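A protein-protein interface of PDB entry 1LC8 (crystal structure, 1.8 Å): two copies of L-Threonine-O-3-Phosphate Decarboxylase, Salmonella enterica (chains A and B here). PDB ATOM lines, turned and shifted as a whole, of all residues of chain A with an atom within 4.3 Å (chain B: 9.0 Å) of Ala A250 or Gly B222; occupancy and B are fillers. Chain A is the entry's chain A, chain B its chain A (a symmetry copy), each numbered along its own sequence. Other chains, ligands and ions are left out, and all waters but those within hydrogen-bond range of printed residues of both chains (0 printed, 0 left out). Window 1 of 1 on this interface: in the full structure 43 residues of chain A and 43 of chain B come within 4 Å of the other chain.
Met B38 touches Ile A53 (CE to CG1, 3.4 Å). Ile A53 touches Leu B46 (CD1 to CD1, 3.7 Å). Ala B219 touches Ile A53. Ile A53 touches Ile B220. Ile A53 touches Leu B223. Pro B221 touches Pro A57 (O to CD, 3.7 Å). Pro A57 touches Arg B224. Gly B222 touches Asn A249 (O to CB, 3.4 Å). CB of Asn A249 touches O of Leu B223 (3.7 Å). Asn A249 touches Arg B224 (CB to CG, 3.9 Å).
The side-chain amide oxygen (OD1) of Asn A249 is in hydrogen-bond range of the backbone NH (N) of Leu A251 (3.1 Å). OD1 of Asn A249 sits at hydrogen-bond distance from N of Ala A252. O of Thr B215 sits at hydrogen-bond distance from N of Ile B220, at 3.1 Å. The backbone carbonyl oxygen (O) of Pro B221 lies within hydrogen-bond range of the guanidinium group (NH1) of Arg B224 (3.1 Å). The backbone carbonyl oxygen (O) of Leu B223 lies within hydrogen-bond range of the side-chain amide nitrogen (ND2) of Asn B249 (2.9 Å). The side-chain amide oxygen (OD1) of Asn B249 is in hydrogen-bond range of the backbone NH (N) of Leu B251 (3.1 Å).
Asn B249 touches its own counterpart, Asn A249. Leu A251 touches its own counterpart, Leu B251. Positions printed for both chains: 249, 251 and 252.
Printed residues of chain B that touch a printed residue of chain A: Met B38, Leu B46, Ala B219, Ile B220, Pro B221, Gly B222, Leu B223, Arg B224, Asn B249 and Leu B251. Hydrophobic or aromatic side chains of chain B that line the printed part of chain A: Met B38, Leu B46, Pro B221, Leu B223 and Leu B251. Printed residues of chain A that touch a printed residue of chain B: Ile A53, Arg A55, Pro A57, Asn A249, Ala A250 and Leu A251. Hydrophobic or aromatic side chains of chain A that line the printed part of chain B: Ile A53, Pro A57, Ala A250 and Leu A251. Among the printed residues, 17 pairs touch across the chains.
Ala A250 touches just one residue of chain B: Gly B222. Ala A252 touches none of the printed residues of chain B. Gly B84 touches none of the printed residues of chain A. Printed residues of chain A within 4 Å of Ile B220: Ile A53 (3.3 Å). Of the printed residues of chain A, Gly B222 touches Ile A53, Arg A55, Asn A249 and Ala A250. Of the printed residues of chain A, Arg B224 touches Pro A57 and Asn A249. The nearest residue of chain B that does not touch Ala A250 is Leu B223 (5.1 Å). The nearest printed residue of chain A that does not touch Gly B222 is Pro A57 (4.01 Å).
The backbone NH of Gly B222 lies within hydrogen-bond range of the backbone carbonyl oxygen of Ile A53, at 2.8 Å. O of Arg A55 lies within hydrogen-bond range of N of Gly B222 (3.1 Å). The side-chain amide nitrogen (ND2) of Asn B249 sits close to the side-chain amide nitrogen (ND2) of Asn A249 (3.2 Å). The backbone NH of Ala A250 sits at hydrogen-bond distance from the backbone carbonyl oxygen of Gly B222. N of Pro B221 lies close to O of Ile A53 (3.2 Å).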
ATOM      1  N   CYS A  52       6.395   3.632  -4.757  1.00  0.00           N
ATOM      2  CA  CYS A  52       6.527   4.113  -3.381  1.00  0.00           C
ATOM      3  C   CYS A  52       5.514   3.433  -2.477  1.00  0.00           C
ATOM      4  O   CYS A  52       5.673   3.444  -1.251  1.00  0.00           O
ATOM      5  CB  CYS A  52       6.377   5.637  -3.289  1.00  0.00           C
ATOM      6  SG  CYS A  52       4.693   6.331  -3.477  1.00  0.00           S
ATOM      7  N   ILE A  53       4.511   2.784  -3.061  1.00  0.00           N
ATOM      8  CA  ILE A  53       3.527   2.133  -2.221  1.00  0.00           C
ATOM      9  C   ILE A  53       4.037   0.820  -1.624  1.00  0.00           C
ATOM     10  O   ILE A  53       3.344   0.199  -0.817  1.00  0.00           O
ATOM     11  CB  ILE A  53       2.208   1.918  -2.960  1.00  0.00           C
ATOM     12  CG1 ILE A  53       2.420   0.983  -4.147  1.00  0.00           C
ATOM     13  CG2 ILE A  53       1.653   3.273  -3.432  1.00  0.00           C
ATOM     14  CD1 ILE A  53       1.093   0.448  -4.708  1.00  0.00           C
ATOM     15  N   ARG A  55       6.383   0.690   0.391  1.00  0.00           N
ATOM     16  CA  ARG A  55       6.884   1.059   1.708  1.00  0.00           C
ATOM     17  C   ARG A  55       5.789   1.826   2.445  1.00  0.00           C
ATOM     18  O   ARG A  55       4.923   2.428   1.807  1.00  0.00           O
ATOM     19  CB  ARG A  55       8.104   1.983   1.559  1.00  0.00           C
ATOM     20  CG  ARG A  55       9.216   1.340   0.718  1.00  0.00           C
ATOM     21  CD  ARG A  55      10.461   2.256   0.578  1.00  0.00           C
ATOM     22  NE  ARG A  55      10.132   3.584   0.050  1.00  0.00           N
ATOM     23  CZ  ARG A  55       9.975   3.887  -1.243  1.00  0.00           C
ATOM     24  NH1 ARG A  55      10.111   2.962  -2.193  1.00  0.00           N
ATOM     25  NH2 ARG A  55       9.692   5.134  -1.591  1.00  0.00           N
ATOM     26  N   PRO A  57       3.971   4.896   4.415  1.00  0.00           N
ATOM     27  CA  PRO A  57       4.122   6.338   4.170  1.00  0.00           C
ATOM     28  C   PRO A  57       5.007   6.847   5.329  1.00  0.00           C
ATOM     29  O   PRO A  57       5.120   6.182   6.372  1.00  0.00           O
ATOM     30  CB  PRO A  57       2.697   6.875   4.348  1.00  0.00           C
ATOM     31  CG  PRO A  57       1.803   5.675   4.097  1.00  0.00           C
ATOM     32  CD  PRO A  57       2.575   4.537   4.707  1.00  0.00           C
ATOM     33  N   VAL A 248      -2.680   8.754   5.994  1.00  0.00           N
ATOM     34  CA  VAL A 248      -2.609   9.363   4.650  1.00  0.00           C
ATOM     35  C   VAL A 248      -1.819   8.417   3.748  1.00  0.00           C
ATOM     36  O   VAL A 248      -0.669   8.056   4.070  1.00  0.00           O
ATOM     37  CB  VAL A 248      -1.926  10.754   4.749  1.00  0.00           C
ATOM     38  CG1 VAL A 248      -1.707  11.355   3.319  1.00  0.00           C
ATOM     39  CG2 VAL A 248      -2.813  11.687   5.594  1.00  0.00           C
ATOM     40  N   ASN A 249      -2.400   7.978   2.634  1.00  0.00           N
ATOM     41  CA  ASN A 249      -1.655   7.040   1.820  1.00  0.00           C
ATOM     42  C   ASN A 249      -0.512   7.740   1.060  1.00  0.00           C
ATOM     43  O   ASN A 249      -0.522   8.957   0.875  1.00  0.00           O
ATOM     44  CB  ASN A 249      -2.594   6.236   0.915  1.00  0.00           C
ATOM     45  CG  ASN A 249      -3.153   7.047  -0.194  1.00  0.00           C
ATOM     46  OD1 ASN A 249      -2.464   7.332  -1.189  1.00  0.00           O
ATOM     47  ND2 ASN A 249      -4.416   7.444  -0.041  1.00  0.00           N
ATOM     48  N   ALA A 250       0.498   6.964   0.665  1.00  0.00           N
ATOM     49  CA  ALA A 250       1.701   7.528   0.050  1.00  0.00           C
ATOM     50  C   ALA A 250       1.434   8.302  -1.229  1.00  0.00           C
ATOM     51  O   ALA A 250       2.099   9.316  -1.505  1.00  0.00           O
ATOM     52  CB  ALA A 250       2.734   6.404  -0.201  1.00  0.00           C
ATOM     53  N   LEU A 251       0.444   7.855  -1.995  1.00  0.00           N
ATOM     54  CA  LEU A 251       0.116   8.537  -3.249  1.00  0.00           C
ATOM     55  C   LEU A 251      -0.625   9.833  -3.001  1.00  0.00           C
ATOM     56  O   LEU A 251      -0.404  10.807  -3.710  1.00  0.00           O
ATOM     57  CB  LEU A 251      -0.683   7.625  -4.170  1.00  0.00           C
ATOM     58  CG  LEU A 251       0.092   6.357  -4.556  1.00  0.00           C
ATOM     59  CD1 LEU A 251      -0.787   5.522  -5.491  1.00  0.00           C
ATOM     60  CD2 LEU A 251       1.439   6.703  -5.224  1.00  0.00           C
ATOM     61  N   ALA A 252      -1.485   9.870  -1.984  1.00  0.00           N
ATOM     62  CA  ALA A 252      -2.165  11.118  -1.663  1.00  0.00           C
ATOM     63  C   ALA A 252      -1.123  12.163  -1.245  1.00  0.00           C
ATOM     64  O   ALA A 252      -1.192  13.328  -1.626  1.00  0.00           O
ATOM     65  CB  ALA A 252      -3.189  10.904  -0.488  1.00  0.00           C
ATOM     66  N   ALA A 253      -0.153  11.752  -0.443  1.00  0.00           N
ATOM     67  CA  ALA A 253       0.843  12.713   0.024  1.00  0.00           C
ATOM     68  C   ALA A 253       1.635  13.292  -1.154  1.00  0.00           C
ATOM     69  O   ALA A 253       1.901  14.487  -1.206  1.00  0.00           O
ATOM     70  CB  ALA A 253       1.784  12.050   1.035  1.00  0.00           C
ATOM     71  N   LEU A 254       2.003  12.422  -2.077  1.00  0.00           N
ATOM     72  CA  LEU A 254       2.760  12.799  -3.277  1.00  0.00           C
ATOM     73  C   LEU A 254       1.936  13.743  -4.135  1.00  0.00           C
ATOM     74  O   LEU A 254       2.407  14.830  -4.521  1.00  0.00           O
ATOM     75  CB  LEU A 254       3.124  11.543  -4.059  1.00  0.00           C
ATOM     76  CG  LEU A 254       3.629  11.692  -5.496  1.00  0.00           C
ATOM     77  CD1 LEU A 254       4.944  12.482  -5.444  1.00  0.00           C
ATOM     78  CD2 LEU A 254       3.821  10.322  -6.157  1.00  0.00           C
ATOM     79  N   ILE B  33       7.970  -6.257   4.773  1.00  0.00           N
ATOM     80  CA  ILE B  33       7.157  -6.288   3.560  1.00  0.00           C
ATOM     81  C   ILE B  33       7.661  -7.341   2.584  1.00  0.00           C
ATOM     82  O   ILE B  33       8.864  -7.459   2.411  1.00  0.00           O
ATOM     83  CB  ILE B  33       7.216  -4.919   2.877  1.00  0.00           C
ATOM     84  CG1 ILE B  33       6.964  -3.791   3.886  1.00  0.00           C
ATOM     85  CG2 ILE B  33       6.217  -4.854   1.750  1.00  0.00           C
ATOM     86  CD1 ILE B  33       5.620  -3.898   4.561  1.00  0.00           C
ATOM     87  N   MET B  38       5.061  -5.454  -5.107  1.00  0.00           N
ATOM     88  CA  MET B  38       3.637  -5.634  -5.383  1.00  0.00           C
ATOM     89  C   MET B  38       3.484  -6.525  -6.610  1.00  0.00           C
ATOM     90  O   MET B  38       4.341  -6.502  -7.493  1.00  0.00           O
ATOM     91  CB  MET B  38       2.950  -4.282  -5.625  1.00  0.00           C
ATOM     92  CG  MET B  38       3.260  -3.617  -6.958  1.00  0.00           C
ATOM     93  SD  MET B  38       2.440  -2.012  -7.239  1.00  0.00           S
ATOM     94  CE  MET B  38       3.743  -0.867  -6.640  1.00  0.00           C
ATOM     95  N   LEU B  46      -3.362  -0.515 -11.440  1.00  0.00           N
ATOM     96  CA  LEU B  46      -3.300   0.834 -10.875  1.00  0.00           C
ATOM     97  C   LEU B  46      -3.002   1.833 -11.972  1.00  0.00           C
ATOM     98  O   LEU B  46      -3.639   2.886 -12.053  1.00  0.00           O
ATOM     99  CB  LEU B  46      -2.216   0.949  -9.798  1.00  0.00           C
ATOM    100  CG  LEU B  46      -2.476   0.204  -8.494  1.00  0.00           C
ATOM    101  CD1 LEU B  46      -1.319   0.403  -7.526  1.00  0.00           C
ATOM    102  CD2 LEU B  46      -3.785   0.715  -7.884  1.00  0.00           C
ATOM    103  N   ASN B  83      -8.696   1.362   6.098  1.00  0.00           N
ATOM    104  CA  ASN B  83      -7.526   2.112   5.578  1.00  0.00           C
ATOM    105  C   ASN B  83      -6.324   1.524   6.326  1.00  0.00           C
ATOM    106  O   ASN B  83      -5.750   2.174   7.203  1.00  0.00           O
ATOM    107  CB  ASN B  83      -7.762   3.586   5.958  1.00  0.00           C
ATOM    108  CG  ASN B  83      -6.695   4.525   5.446  1.00  0.00           C
ATOM    109  OD1 ASN B  83      -6.316   5.495   6.129  1.00  0.00           O
ATOM    110  ND2 ASN B  83      -6.240   4.284   4.239  1.00  0.00           N
ATOM    111  N   GLY B  84      -5.951   0.301   5.927  1.00  0.00           N
ATOM    112  CA  GLY B  84      -4.907  -0.460   6.568  1.00  0.00           C
ATOM    113  C   GLY B  84      -5.596  -1.256   7.676  1.00  0.00           C
ATOM    114  O   GLY B  84      -6.669  -0.845   8.129  1.00  0.00           O
ATOM    115  N   LEU B 214      -3.507  -6.622   4.009  1.00  0.00           N
ATOM    116  CA  LEU B 214      -2.946  -6.998   2.713  1.00  0.00           C
ATOM    117  C   LEU B 214      -1.600  -6.282   2.496  1.00  0.00           C
ATOM    118  O   LEU B 214      -0.887  -6.564   1.521  1.00  0.00           O
ATOM    119  CB  LEU B 214      -3.869  -6.576   1.565  1.00  0.00           C
ATOM    120  CG  LEU B 214      -4.899  -7.619   1.155  1.00  0.00           C
ATOM    121  CD1 LEU B 214      -6.144  -7.393   1.980  1.00  0.00           C
ATOM    122  CD2 LEU B 214      -5.241  -7.415  -0.320  1.00  0.00           C
ATOM    123  N   THR B 215      -1.202  -5.407   3.414  1.00  0.00           N
ATOM    124  CA  THR B 215       0.000  -4.633   3.130  1.00  0.00           C
ATOM    125  C   THR B 215       1.346  -5.347   3.161  1.00  0.00           C
ATOM    126  O   THR B 215       2.227  -5.032   2.342  1.00  0.00           O
ATOM    127  CB  THR B 215       0.066  -3.358   3.988  1.00  0.00           C
ATOM    128  OG1 THR B 215       0.146  -3.732   5.360  1.00  0.00           O
ATOM    129  CG2 THR B 215      -1.198  -2.466   3.728  1.00  0.00           C
ATOM    130  N   LYS B 216       1.525  -6.309   4.048  1.00  0.00           N
ATOM    131  CA  LYS B 216       2.810  -7.005   4.075  1.00  0.00           C
ATOM    132  C   LYS B 216       2.903  -8.096   3.004  1.00  0.00           C
ATOM    133  O   LYS B 216       3.880  -8.164   2.240  1.00  0.00           O
ATOM    134  CB  LYS B 216       3.058  -7.621   5.452  1.00  0.00           C
ATOM    135  CG  LYS B 216       2.993  -6.594   6.594  1.00  0.00           C
ATOM    136  CD  LYS B 216       1.667  -6.769   7.353  1.00  0.00           C
ATOM    137  CE  LYS B 216       1.370  -5.585   8.300  1.00  0.00           C
ATOM    138  NZ  LYS B 216       2.601  -5.078   8.966  1.00  0.00           N
ATOM    139  N   TYR B 218       1.182  -8.557   0.191  1.00  0.00           N
ATOM    140  CA  TYR B 218       1.110  -8.126  -1.203  1.00  0.00           C
ATOM    141  C   TYR B 218       1.933  -6.872  -1.437  1.00  0.00           C
ATOM    142  O   TYR B 218       1.849  -6.298  -2.494  1.00  0.00           O
ATOM    143  CB  TYR B 218      -0.345  -7.873  -1.614  1.00  0.00           C
ATOM    144  CG  TYR B 218      -1.182  -9.113  -1.599  1.00  0.00           C
ATOM    145  CD1 TYR B 218      -2.105  -9.343  -0.582  1.00  0.00           C
ATOM    146  CD2 TYR B 218      -1.048 -10.071  -2.610  1.00  0.00           C
ATOM    147  CE1 TYR B 218      -2.880 -10.497  -0.576  1.00  0.00           C
ATOM    148  CE2 TYR B 218      -1.814 -11.230  -2.611  1.00  0.00           C
ATOM    149  CZ  TYR B 218      -2.717 -11.435  -1.611  1.00  0.00           C
ATOM    150  OH  TYR B 218      -3.486 -12.569  -1.664  1.00  0.00           O
ATOM    151  N   ALA B 219       2.688  -6.436  -0.427  1.00  0.00           N
ATOM    152  CA  ALA B 219       3.561  -5.282  -0.550  1.00  0.00           C
ATOM    153  C   ALA B 219       2.949  -3.964  -0.982  1.00  0.00           C
ATOM    154  O   ALA B 219       3.457  -3.323  -1.919  1.00  0.00           O
ATOM    155  CB  ALA B 219       4.727  -5.629  -1.518  1.00  0.00           C
ATOM    156  N   ILE B 220       1.859  -3.562  -0.326  1.00  0.00           N
ATOM    157  CA  ILE B 220       1.222  -2.283  -0.621  1.00  0.00           C
ATOM    158  C   ILE B 220       1.004  -1.497   0.677  1.00  0.00           C
ATOM    159  O   ILE B 220      -0.059  -0.892   0.863  1.00  0.00           O
ATOM    160  CB  ILE B 220      -0.163  -2.498  -1.322  1.00  0.00           C
ATOM    161  CG1 ILE B 220      -1.075  -3.380  -0.482  1.00  0.00           C
ATOM    162  CG2 ILE B 220       0.041  -3.150  -2.702  1.00  0.00           C
ATOM    163  CD1 ILE B 220      -2.505  -3.469  -1.120  1.00  0.00           C
ATOM    164  N   PRO B 221       1.999  -1.494   1.591  1.00  0.00           N
ATOM    165  CA  PRO B 221       1.823  -0.753   2.855  1.00  0.00           C
ATOM    166  C   PRO B 221       1.622   0.744   2.630  1.00  0.00           C
ATOM    167  O   PRO B 221       1.037   1.433   3.465  1.00  0.00           O
ATOM    168  CB  PRO B 221       3.110  -1.063   3.617  1.00  0.00           C
ATOM    169  CG  PRO B 221       4.130  -1.176   2.517  1.00  0.00           C
ATOM    170  CD  PRO B 221       3.357  -2.065   1.530  1.00  0.00           C
ATOM    171  N   GLY B 222       2.095   1.256   1.497  1.00  0.00           N
ATOM    172  CA  GLY B 222       1.886   2.679   1.222  1.00  0.00           C
ATOM    173  C   GLY B 222       0.468   3.001   0.724  1.00  0.00           C
ATOM    174  O   GLY B 222       0.040   4.176   0.702  1.00  0.00           O
ATOM    175  N   LEU B 223      -0.265   1.969   0.311  1.00  0.00           N
ATOM    176  CA  LEU B 223      -1.621   2.174  -0.206  1.00  0.00           C
ATOM    177  C   LEU B 223      -2.642   2.089   0.899  1.00  0.00           C
ATOM    178  O   LEU B 223      -3.700   2.719   0.798  1.00  0.00           O
ATOM    179  CB  LEU B 223      -1.973   1.157  -1.296  1.00  0.00           C
ATOM    180  CG  LEU B 223      -1.960   1.606  -2.774  1.00  0.00           C
ATOM    181  CD1 LEU B 223      -2.613   0.526  -3.602  1.00  0.00           C
ATOM    182  CD2 LEU B 223      -2.753   2.910  -2.959  1.00  0.00           C
ATOM    183  N   ARG B 224      -2.305   1.307   1.929  1.00  0.00           N
ATOM    184  CA  ARG B 224      -3.136   1.098   3.131  1.00  0.00           C
ATOM    185  C   ARG B 224      -4.393   0.242   2.901  1.00  0.00           C
ATOM    186  O   ARG B 224      -5.389   0.734   2.395  1.00  0.00           O
ATOM    187  CB  ARG B 224      -3.562   2.459   3.719  1.00  0.00           C
ATOM    188  CG  ARG B 224      -2.495   3.601   3.735  1.00  0.00           C
ATOM    189  CD  ARG B 224      -1.281   3.251   4.615  1.00  0.00           C
ATOM    190  NE  ARG B 224      -1.678   2.888   5.986  1.00  0.00           N
ATOM    191  CZ  ARG B 224      -1.444   1.693   6.530  1.00  0.00           C
ATOM    192  NH1 ARG B 224      -0.806   0.769   5.832  1.00  0.00           N
ATOM    193  NH2 ARG B 224      -1.869   1.397   7.761  1.00  0.00           N
ATOM    194  N   LEU B 225      -4.351  -1.034   3.266  1.00  0.00           N
ATOM    195  CA  LEU B 225      -5.548  -1.838   3.107  1.00  0.00           C
ATOM    196  C   LEU B 225      -5.533  -3.016   4.052  1.00  0.00           C
ATOM    197  O   LEU B 225      -4.574  -3.798   4.093  1.00  0.00           O
ATOM    198  CB  LEU B 225      -5.710  -2.335   1.668  1.00  0.00           C
ATOM    199  CG  LEU B 225      -7.004  -3.135   1.434  1.00  0.00           C
ATOM    200  CD1 LEU B 225      -8.226  -2.183   1.583  1.00  0.00           C
ATOM    201  CD2 LEU B 225      -7.005  -3.750  -0.003  1.00  0.00           C
ATOM    202  N   ASN B 249      -9.016   4.312   0.177  1.00  0.00           N
ATOM    203  CA  ASN B 249      -8.890   5.053  -1.061  1.00  0.00           C
ATOM    204  C   ASN B 249      -9.192   4.162  -2.282  1.00  0.00           C
ATOM    205  O   ASN B 249      -9.137   2.935  -2.204  1.00  0.00           O
ATOM    206  CB  ASN B 249      -7.534   5.762  -1.137  1.00  0.00           C
ATOM    207  CG  ASN B 249      -6.409   4.823  -1.362  1.00  0.00           C
ATOM    208  OD1 ASN B 249      -6.198   4.334  -2.486  1.00  0.00           O
ATOM    209  ND2 ASN B 249      -5.665   4.544  -0.293  1.00  0.00           N
ATOM    210  N   LEU B 251      -7.685   3.490  -5.027  1.00  0.00           N
ATOM    211  CA  LEU B 251      -6.609   2.639  -5.538  1.00  0.00           C
ATOM    212  C   LEU B 251      -6.358   1.453  -4.630  1.00  0.00           C
ATOM    213  O   LEU B 251      -6.074   0.365  -5.114  1.00  0.00           O
ATOM    214  CB  LEU B 251      -5.332   3.443  -5.742  1.00  0.00           C
ATOM    215  CG  LEU B 251      -5.509   4.576  -6.763  1.00  0.00           C
ATOM    216  CD1 LEU B 251      -4.172   5.307  -6.908  1.00  0.00           C
ATOM    217  CD2 LEU B 251      -5.995   4.035  -8.124  1.00  0.00           C
ATOM    218  N   ALA B 252      -6.488   1.640  -3.317  1.00  0.00           N
ATOM    219  CA  ALA B 252      -6.328   0.510  -2.412  1.00  0.00           C
ATOM    220  C   ALA B 252      -7.425  -0.523  -2.702  1.00  0.00           C
ATOM    221  O   ALA B 252      -7.184  -1.727  -2.724  1.00  0.00           O
ATOM    222  CB  ALA B 252      -6.439   0.981  -0.914  1.00  0.00           C
